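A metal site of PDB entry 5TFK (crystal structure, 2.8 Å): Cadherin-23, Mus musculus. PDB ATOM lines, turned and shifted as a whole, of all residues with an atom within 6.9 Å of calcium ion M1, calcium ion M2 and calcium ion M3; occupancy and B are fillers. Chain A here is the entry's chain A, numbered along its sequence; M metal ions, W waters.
Of the 27 residues printed, 5 come within 4 Å of calcium ion M1. The nearest printed residue that does not touch calcium ion M1 is His 323 (4.1 Å).
Within 4 Å of calcium ion M3: Glu 133, Asp 186, Glu 188 and Asp 222.
Calcium ion M3 is bound by water W1, OD1 of Asp 186, OE2 of Glu 188, OD1 of Asp 222, OD2 of Asp 222 and OE1 of Glu 133. Calcium ion M3 has six donor atoms within binding distance.
Calcium ion M1 is bound by the backbone carbonyl oxygen (O) of Ser 223 (2.1 Å). OD2 of Asp 315 is bound to calcium ion M1, at 2.4 Å. OD1 of Asp 253 binds calcium ion M1 (2.4 Å). Calcium ion M1 is bound by OD1 of Asn 221 (2.5 Å). OD2 of Asp 253 binds calcium ion M1, at 2.6 Å. The side-chain carboxylate (OD2) of Asp 255 binds calcium ion M1 (2.6 Å).
ND1 of His 323 sits at hydrogen-bond distance from O of Asp 222 (2.7 Å). OD2 of Asp 222 lies close to ND2 of Asn 134 (2.8 Å). The side-chain carboxylate (OD1) of Asp 315 sits at hydrogen-bond distance from the backbone NH (N) of Ala 317 (3.2 Å). The backbone carbonyl oxygen (O) of Ala 317 sits at hydrogen-bond distance from the side-chain amide nitrogen (ND2) of Asn 221 (3.5 Å). N of Asn 221 lies within hydrogen-bond range of OD2 of Asp 319. The side-chain carboxylate (OE1) of Glu 133 lies close to the backbone NH (N) of Arg 187 (3.2 Å). OD2 of Asp 219 sits at hydrogen-bond distance from N of Leu 256, at 3.4 Å. The side-chain carboxylate of Asp 219 lies close to the guanidinium group of Arg 187 (3.0 Å).
Calcium ion M2 is bound by OE2 of Glu 188. Calcium ion M2 is bound by the backbone carbonyl oxygen (O) of Ile 220, at 2.3 Å. Calcium ion M2 is bound by the side-chain carboxylate (OD1) of Asp 255 (2.3 Å). OD1 of Asp 219 is bound to calcium ion M2 (2.3 Å). The side-chain carboxylate (OE2) of Glu 133 is bound to calcium ion M2 (2.3 Å). Calcium ion M2 is bound by the side-chain carboxylate (OD1) of Asp 222 (2.6 Å). Calcium ion M2 is bound by OE1 of Glu 188, 2.8 Å away. Calcium ion M2 has seven donor atoms within binding distance.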
ATOM      1  N   GLU A 133     -10.993  14.706  -4.762  1.00  0.00           N
ATOM      2  CA  GLU A 133     -11.185  15.249  -6.120  1.00  0.00           C
ATOM      3  C   GLU A 133     -12.281  14.566  -6.967  1.00  0.00           C
ATOM      4  O   GLU A 133     -12.797  13.477  -6.629  1.00  0.00           O
ATOM      5  CB  GLU A 133      -9.855  15.287  -6.914  1.00  0.00           C
ATOM      6  CG  GLU A 133      -9.292  13.934  -7.373  1.00  0.00           C
ATOM      7  CD  GLU A 133      -8.107  14.033  -8.333  1.00  0.00           C
ATOM      8  OE1 GLU A 133      -8.206  14.712  -9.372  1.00  0.00           O
ATOM      9  OE2 GLU A 133      -7.083  13.377  -8.095  1.00  0.00           O
ATOM     10  N   ASN A 134     -12.612  15.239  -8.083  1.00  0.00           N
ATOM     11  CA  ASN A 134     -13.705  14.852  -8.999  1.00  0.00           C
ATOM     12  C   ASN A 134     -15.051  14.771  -8.286  1.00  0.00           C
ATOM     13  O   ASN A 134     -15.804  13.811  -8.407  1.00  0.00           O
ATOM     14  CB  ASN A 134     -13.409  13.503  -9.668  1.00  0.00           C
ATOM     15  CG  ASN A 134     -12.102  13.499 -10.394  1.00  0.00           C
ATOM     16  OD1 ASN A 134     -11.843  14.390 -11.195  1.00  0.00           O
ATOM     17  ND2 ASN A 134     -11.275  12.498 -10.114  1.00  0.00           N
ATOM     18  N   ILE A 185     -13.064  19.851  -9.652  1.00  0.00           N
ATOM     19  CA  ILE A 185     -11.937  19.899  -8.729  1.00  0.00           C
ATOM     20  C   ILE A 185     -10.937  18.841  -9.098  1.00  0.00           C
ATOM     21  O   ILE A 185     -11.122  17.673  -8.759  1.00  0.00           O
ATOM     22  CB  ILE A 185     -12.389  19.652  -7.277  1.00  0.00           C
ATOM     23  CG1 ILE A 185     -13.334  20.772  -6.820  1.00  0.00           C
ATOM     24  CG2 ILE A 185     -11.209  19.507  -6.314  1.00  0.00           C
ATOM     25  CD1 ILE A 185     -12.862  22.179  -7.148  1.00  0.00           C
ATOM     26  N   ASP A 186      -9.888  19.246  -9.812  1.00  0.00           N
ATOM     27  CA  ASP A 186      -8.828  18.331 -10.231  1.00  0.00           C
ATOM     28  C   ASP A 186      -7.615  18.598  -9.378  1.00  0.00           C
ATOM     29  O   ASP A 186      -7.054  19.681  -9.462  1.00  0.00           O
ATOM     30  CB  ASP A 186      -8.477  18.607 -11.696  1.00  0.00           C
ATOM     31  CG  ASP A 186      -7.478  17.615 -12.263  1.00  0.00           C
ATOM     32  OD1 ASP A 186      -7.091  16.663 -11.571  1.00  0.00           O
ATOM     33  OD2 ASP A 186      -7.087  17.803 -13.440  1.00  0.00           O
ATOM     34  N   ARG A 187      -7.219  17.610  -8.580  1.00  0.00           N
ATOM     35  CA  ARG A 187      -5.996  17.707  -7.778  1.00  0.00           C
ATOM     36  C   ARG A 187      -4.747  18.004  -8.586  1.00  0.00           C
ATOM     37  O   ARG A 187      -3.826  18.646  -8.085  1.00  0.00           O
ATOM     38  CB  ARG A 187      -5.734  16.409  -7.021  1.00  0.00           C
ATOM     39  CG  ARG A 187      -4.874  16.603  -5.776  1.00  0.00           C
ATOM     40  CD  ARG A 187      -4.264  15.302  -5.318  1.00  0.00           C
ATOM     41  NE  ARG A 187      -3.272  14.895  -6.305  1.00  0.00           N
ATOM     42  CZ  ARG A 187      -1.995  15.244  -6.291  1.00  0.00           C
ATOM     43  NH1 ARG A 187      -1.479  15.960  -5.288  1.00  0.00           N
ATOM     44  NH2 ARG A 187      -1.214  14.816  -7.278  1.00  0.00           N
ATOM     45  N   GLU A 188      -4.699  17.512  -9.814  1.00  0.00           N
ATOM     46  CA  GLU A 188      -3.573  17.784 -10.708  1.00  0.00           C
ATOM     47  C   GLU A 188      -3.567  19.240 -11.223  1.00  0.00           C
ATOM     48  O   GLU A 188      -2.515  19.743 -11.616  1.00  0.00           O
ATOM     49  CB  GLU A 188      -3.575  16.792 -11.869  1.00  0.00           C
ATOM     50  CG  GLU A 188      -3.001  15.416 -11.543  1.00  0.00           C
ATOM     51  CD  GLU A 188      -3.800  14.625 -10.525  1.00  0.00           C
ATOM     52  OE1 GLU A 188      -3.374  14.491  -9.350  1.00  0.00           O
ATOM     53  OE2 GLU A 188      -4.865  14.089 -10.893  1.00  0.00           O
ATOM     54  N   GLU A 189      -4.725  19.898 -11.217  1.00  0.00           N
ATOM     55  CA  GLU A 189      -4.801  21.337 -11.522  1.00  0.00           C
ATOM     56  C   GLU A 189      -4.358  22.183 -10.331  1.00  0.00           C
ATOM     57  O   GLU A 189      -3.642  23.170 -10.480  1.00  0.00           O
ATOM     58  CB  GLU A 189      -6.226  21.748 -11.953  1.00  0.00           C
ATOM     59  CG  GLU A 189      -6.393  23.241 -12.219  1.00  0.00           C
ATOM     60  CD  GLU A 189      -7.654  23.578 -12.977  1.00  0.00           C
ATOM     61  OE1 GLU A 189      -7.581  24.423 -13.887  1.00  0.00           O
ATOM     62  OE2 GLU A 189      -8.724  23.017 -12.647  1.00  0.00           O
ATOM     63  N   ASP A 218      -7.582  15.366  -2.023  1.00  0.00           N
ATOM     64  CA  ASP A 218      -7.041  14.046  -1.889  1.00  0.00           C
ATOM     65  C   ASP A 218      -7.062  13.502  -3.286  1.00  0.00           C
ATOM     66  O   ASP A 218      -7.837  13.955  -4.134  1.00  0.00           O
ATOM     67  CB  ASP A 218      -7.872  13.208  -0.925  1.00  0.00           C
ATOM     68  CG  ASP A 218      -7.595  13.559   0.506  1.00  0.00           C
ATOM     69  OD1 ASP A 218      -6.748  14.443   0.736  1.00  0.00           O
ATOM     70  OD2 ASP A 218      -8.201  12.971   1.415  1.00  0.00           O
ATOM     71  N   ASP A 219      -6.185  12.549  -3.553  1.00  0.00           N
ATOM     72  CA  ASP A 219      -5.946  12.058  -4.918  1.00  0.00           C
ATOM     73  C   ASP A 219      -6.799  10.831  -5.242  1.00  0.00           C
ATOM     74  O   ASP A 219      -6.922   9.908  -4.439  1.00  0.00           O
ATOM     75  CB  ASP A 219      -4.473  11.745  -5.079  1.00  0.00           C
ATOM     76  CG  ASP A 219      -4.108  11.374  -6.478  1.00  0.00           C
ATOM     77  OD1 ASP A 219      -4.225  12.221  -7.386  1.00  0.00           O
ATOM     78  OD2 ASP A 219      -3.704  10.209  -6.665  1.00  0.00           O
ATOM     79  N   ILE A 220      -7.448  10.898  -6.399  1.00  0.00           N
ATOM     80  CA  ILE A 220      -7.813   9.698  -7.119  1.00  0.00           C
ATOM     81  C   ILE A 220      -6.758   9.592  -8.226  1.00  0.00           C
ATOM     82  O   ILE A 220      -6.348  10.602  -8.800  1.00  0.00           O
ATOM     83  CB  ILE A 220      -9.232   9.792  -7.727  1.00  0.00           C
ATOM     84  CG1 ILE A 220     -10.294  10.047  -6.647  1.00  0.00           C
ATOM     85  CG2 ILE A 220      -9.562   8.505  -8.460  1.00  0.00           C
ATOM     86  CD1 ILE A 220     -11.652  10.477  -7.202  1.00  0.00           C
ATOM     87  N   ASN A 221      -6.294   8.366  -8.490  1.00  0.00           N
ATOM     88  CA  ASN A 221      -5.390   8.114  -9.611  1.00  0.00           C
ATOM     89  C   ASN A 221      -6.172   8.145 -10.921  1.00  0.00           C
ATOM     90  O   ASN A 221      -6.610   7.115 -11.437  1.00  0.00           O
ATOM     91  CB  ASN A 221      -4.668   6.783  -9.435  1.00  0.00           C
ATOM     92  CG  ASN A 221      -3.535   6.614 -10.411  1.00  0.00           C
ATOM     93  OD1 ASN A 221      -3.710   6.817 -11.612  1.00  0.00           O
ATOM     94  ND2 ASN A 221      -2.362   6.269  -9.911  1.00  0.00           N
ATOM     95  N   ASP A 222      -6.370   9.340 -11.447  1.00  0.00           N
ATOM     96  CA  ASP A 222      -7.314   9.565 -12.517  1.00  0.00           C
ATOM     97  C   ASP A 222      -6.656  10.182 -13.721  1.00  0.00           C
ATOM     98  O   ASP A 222      -7.338  10.610 -14.641  1.00  0.00           O
ATOM     99  CB  ASP A 222      -8.462  10.471 -12.019  1.00  0.00           C
ATOM    100  CG  ASP A 222      -7.990  11.875 -11.651  1.00  0.00           C
ATOM    101  OD1 ASP A 222      -6.786  12.103 -11.430  1.00  0.00           O
ATOM    102  OD2 ASP A 222      -8.852  12.753 -11.555  1.00  0.00           O
ATOM    103  N   SER A 223      -5.329  10.195 -13.727  1.00  0.00           N
ATOM    104  CA  SER A 223      -4.584  10.963 -14.705  1.00  0.00           C
ATOM    105  C   SER A 223      -3.697  10.009 -15.491  1.00  0.00           C
ATOM    106  O   SER A 223      -2.910   9.271 -14.900  1.00  0.00           O
ATOM    107  CB  SER A 223      -3.738  12.013 -14.002  1.00  0.00           C
ATOM    108  OG  SER A 223      -3.454  13.080 -14.862  1.00  0.00           O
ATOM    109  N   ARG A 224      -3.876   9.994 -16.814  1.00  0.00           N
ATOM    110  CA  ARG A 224      -3.186   9.041 -17.675  1.00  0.00           C
ATOM    111  C   ARG A 224      -1.707   9.390 -17.869  1.00  0.00           C
ATOM    112  O   ARG A 224      -1.352  10.556 -18.036  1.00  0.00           O
ATOM    113  CB  ARG A 224      -3.884   8.902 -19.037  1.00  0.00           C
ATOM    114  CG  ARG A 224      -3.562   9.995 -20.055  1.00  0.00           C
ATOM    115  CD  ARG A 224      -4.081   9.662 -21.450  1.00  0.00           C
ATOM    116  NE  ARG A 224      -5.529   9.840 -21.610  1.00  0.00           N
ATOM    117  CZ  ARG A 224      -6.438   8.877 -21.516  1.00  0.00           C
ATOM    118  NH1 ARG A 224      -6.104   7.624 -21.224  1.00  0.00           N
ATOM    119  NH2 ARG A 224      -7.720   9.177 -21.699  1.00  0.00           N
ATOM    120  N   PRO A 225      -0.849   8.371 -17.898  1.00  0.00           N
ATOM    121  CA  PRO A 225       0.551   8.644 -18.224  1.00  0.00           C
ATOM    122  C   PRO A 225       0.727   9.242 -19.615  1.00  0.00           C
ATOM    123  O   PRO A 225       0.018   8.914 -20.590  1.00  0.00           O
ATOM    124  CB  PRO A 225       1.223   7.267 -18.085  1.00  0.00           C
ATOM    125  CG  PRO A 225       0.139   6.263 -18.202  1.00  0.00           C
ATOM    126  CD  PRO A 225      -1.097   6.934 -17.707  1.00  0.00           C
ATOM    127  N   ASP A 253       3.471  10.668 -14.998  1.00  0.00           N
ATOM    128  CA  ASP A 253       2.121  10.551 -14.422  1.00  0.00           C
ATOM    129  C   ASP A 253       1.992  11.450 -13.181  1.00  0.00           C
ATOM    130  O   ASP A 253       2.801  11.376 -12.289  1.00  0.00           O
ATOM    131  CB  ASP A 253       1.851   9.096 -14.017  1.00  0.00           C
ATOM    132  CG  ASP A 253       0.352   8.740 -13.955  1.00  0.00           C
ATOM    133  OD1 ASP A 253      -0.359   9.106 -13.003  1.00  0.00           O
ATOM    134  OD2 ASP A 253      -0.099   7.989 -14.835  1.00  0.00           O
ATOM    135  N   LEU A 254       0.992  12.319 -13.192  1.00  0.00           N
ATOM    136  CA  LEU A 254       0.898  13.399 -12.225  1.00  0.00           C
ATOM    137  C   LEU A 254       0.113  13.023 -10.972  1.00  0.00           C
ATOM    138  O   LEU A 254      -0.033  13.841 -10.074  1.00  0.00           O
ATOM    139  CB  LEU A 254       0.260  14.625 -12.874  1.00  0.00           C
ATOM    140  CG  LEU A 254       1.009  15.157 -14.096  1.00  0.00           C
ATOM    141  CD1 LEU A 254       0.102  16.041 -14.950  1.00  0.00           C
ATOM    142  CD2 LEU A 254       2.264  15.891 -13.659  1.00  0.00           C
ATOM    143  N   ASP A 255      -0.376  11.788 -10.893  1.00  0.00           N
ATOM    144  CA  ASP A 255      -1.032  11.295  -9.694  1.00  0.00           C
ATOM    145  C   ASP A 255       0.008  10.952  -8.636  1.00  0.00           C
ATOM    146  O   ASP A 255       1.204  10.997  -8.903  1.00  0.00           O
ATOM    147  CB  ASP A 255      -1.899  10.067 -10.015  1.00  0.00           C
ATOM    148  CG  ASP A 255      -3.066  10.400 -10.916  1.00  0.00           C
ATOM    149  OD1 ASP A 255      -3.847  11.323 -10.579  1.00  0.00           O
ATOM    150  OD2 ASP A 255      -3.215   9.714 -11.962  1.00  0.00           O
ATOM    151  N   LEU A 256      -0.457  10.570  -7.449  1.00  0.00           N
ATOM    152  CA  LEU A 256       0.397  10.530  -6.287  1.00  0.00           C
ATOM    153  C   LEU A 256       1.320   9.326  -6.222  1.00  0.00           C
ATOM    154  O   LEU A 256       2.445   9.476  -5.772  1.00  0.00           O
ATOM    155  CB  LEU A 256      -0.407  10.680  -4.992  1.00  0.00           C
ATOM    156  CG  LEU A 256      -0.505  12.120  -4.459  1.00  0.00           C
ATOM    157  CD1 LEU A 256      -1.483  12.231  -3.307  1.00  0.00           C
ATOM    158  CD2 LEU A 256       0.846  12.664  -4.006  1.00  0.00           C
ATOM    159  N   PRO A 258       2.154   6.473  -8.865  1.00  0.00           N
ATOM    160  CA  PRO A 258       2.066   5.651 -10.064  1.00  0.00           C
ATOM    161  C   PRO A 258       2.992   4.456  -9.984  1.00  0.00           C
ATOM    162  O   PRO A 258       4.013   4.509  -9.296  1.00  0.00           O
ATOM    163  CB  PRO A 258       2.508   6.599 -11.179  1.00  0.00           C
ATOM    164  CG  PRO A 258       3.191   7.724 -10.508  1.00  0.00           C
ATOM    165  CD  PRO A 258       2.563   7.852  -9.163  1.00  0.00           C
ATOM    166  N   LEU A 260       4.494   2.775 -13.247  1.00  0.00           N
ATOM    167  CA  LEU A 260       4.512   2.837 -14.687  1.00  0.00           C
ATOM    168  C   LEU A 260       5.206   1.595 -15.253  1.00  0.00           C
ATOM    169  O   LEU A 260       6.309   1.229 -14.829  1.00  0.00           O
ATOM    170  CB  LEU A 260       5.209   4.103 -15.164  1.00  0.00           C
ATOM    171  CG  LEU A 260       4.540   5.443 -14.802  1.00  0.00           C
ATOM    172  CD1 LEU A 260       5.175   6.620 -15.544  1.00  0.00           C
ATOM    173  CD2 LEU A 260       3.063   5.415 -15.094  1.00  0.00           C
ATOM    174  N   ASP A 315      -0.240   2.989 -16.132  1.00  0.00           N
ATOM    175  CA  ASP A 315      -0.206   3.138 -14.666  1.00  0.00           C
ATOM    176  C   ASP A 315      -0.963   1.990 -14.010  1.00  0.00           C
ATOM    177  O   ASP A 315      -2.145   1.869 -14.250  1.00  0.00           O
ATOM    178  CB  ASP A 315      -0.861   4.479 -14.307  1.00  0.00           C
ATOM    179  CG  ASP A 315      -0.547   4.935 -12.889  1.00  0.00           C
ATOM    180  OD1 ASP A 315      -0.011   4.121 -12.107  1.00  0.00           O
ATOM    181  OD2 ASP A 315      -0.846   6.119 -12.546  1.00  0.00           O
ATOM    182  N   ALA A 317      -1.452   1.563 -10.902  1.00  0.00           N
ATOM    183  CA  ALA A 317      -2.139   2.044  -9.730  1.00  0.00           C
ATOM    184  C   ALA A 317      -3.401   2.782 -10.143  1.00  0.00           C
ATOM    185  O   ALA A 317      -4.087   3.330  -9.282  1.00  0.00           O
ATOM    186  CB  ALA A 317      -1.226   2.950  -8.938  1.00  0.00           C
ATOM    187  N   SER A 318      -3.738   2.788 -11.420  1.00  0.00           N
ATOM    188  CA  SER A 318      -4.840   3.630 -11.884  1.00  0.00           C
ATOM    189  C   SER A 318      -6.165   3.182 -11.283  1.00  0.00           C
ATOM    190  O   SER A 318      -6.406   1.987 -11.084  1.00  0.00           O
ATOM    191  CB  SER A 318      -4.894   3.674 -13.411  1.00  0.00           C
ATOM    192  OG  SER A 318      -5.409   4.926 -13.862  1.00  0.00           O
ATOM    193  N   ASP A 319      -6.976   4.171 -10.920  1.00  0.00           N
ATOM    194  CA  ASP A 319      -8.239   3.931 -10.230  1.00  0.00           C
ATOM    195  C   ASP A 319      -9.391   3.942 -11.223  1.00  0.00           C
ATOM    196  O   ASP A 319     -10.433   3.364 -10.964  1.00  0.00           O
ATOM    197  CB  ASP A 319      -8.472   4.974  -9.134  1.00  0.00           C
ATOM    198  CG  ASP A 319      -7.630   4.726  -7.875  1.00  0.00           C
ATOM    199  OD1 ASP A 319      -7.735   3.628  -7.261  1.00  0.00           O
ATOM    200  OD2 ASP A 319      -6.879   5.639  -7.469  1.00  0.00           O
ATOM    201  N   HIS A 323      -8.306   6.116 -17.827  1.00  0.00           N
ATOM    202  CA  HIS A 323      -7.184   7.075 -17.751  1.00  0.00           C
ATOM    203  C   HIS A 323      -5.894   6.386 -17.270  1.00  0.00           C
ATOM    204  O   HIS A 323      -5.152   6.904 -16.406  1.00  0.00           O
ATOM    205  CB  HIS A 323      -7.518   8.233 -16.801  1.00  0.00           C
ATOM    206  CG  HIS A 323      -8.567   9.169 -17.309  1.00  0.00           C
ATOM    207  ND1 HIS A 323      -9.198  10.100 -16.509  1.00  0.00           N
ATOM    208  CD2 HIS A 323      -9.106   9.320 -18.544  1.00  0.00           C
ATOM    209  CE1 HIS A 323     -10.070  10.781 -17.221  1.00  0.00           C
ATOM    210  NE2 HIS A 323     -10.037  10.333 -18.461  1.00  0.00           N
ATOM    211  N   SER A 324      -5.643   5.204 -17.822  1.00  0.00           N
ATOM    212  CA  SER A 324      -4.585   4.355 -17.303  1.00  0.00           C
ATOM    213  C   SER A 324      -3.553   3.957 -18.332  1.00  0.00           C
ATOM    214  O   SER A 324      -2.533   3.439 -17.946  1.00  0.00           O
ATOM    215  CB  SER A 324      -5.179   3.086 -16.690  1.00  0.00           C
ATOM    216  OG  SER A 324      -5.640   2.234 -17.698  1.00  0.00           O
HETATM  217 CA    CA M   1      -2.327   7.770 -13.505  1.00  0.00          CA
HETATM  218 CA    CA M   2      -5.344  12.543  -9.362  1.00  0.00          CA
HETATM  219 CA    CA M   3      -7.066  14.482 -11.600  1.00  0.00          CA
HETATM  220  O   HOH W   1      -9.109  15.105 -11.340  1.00  0.00           O
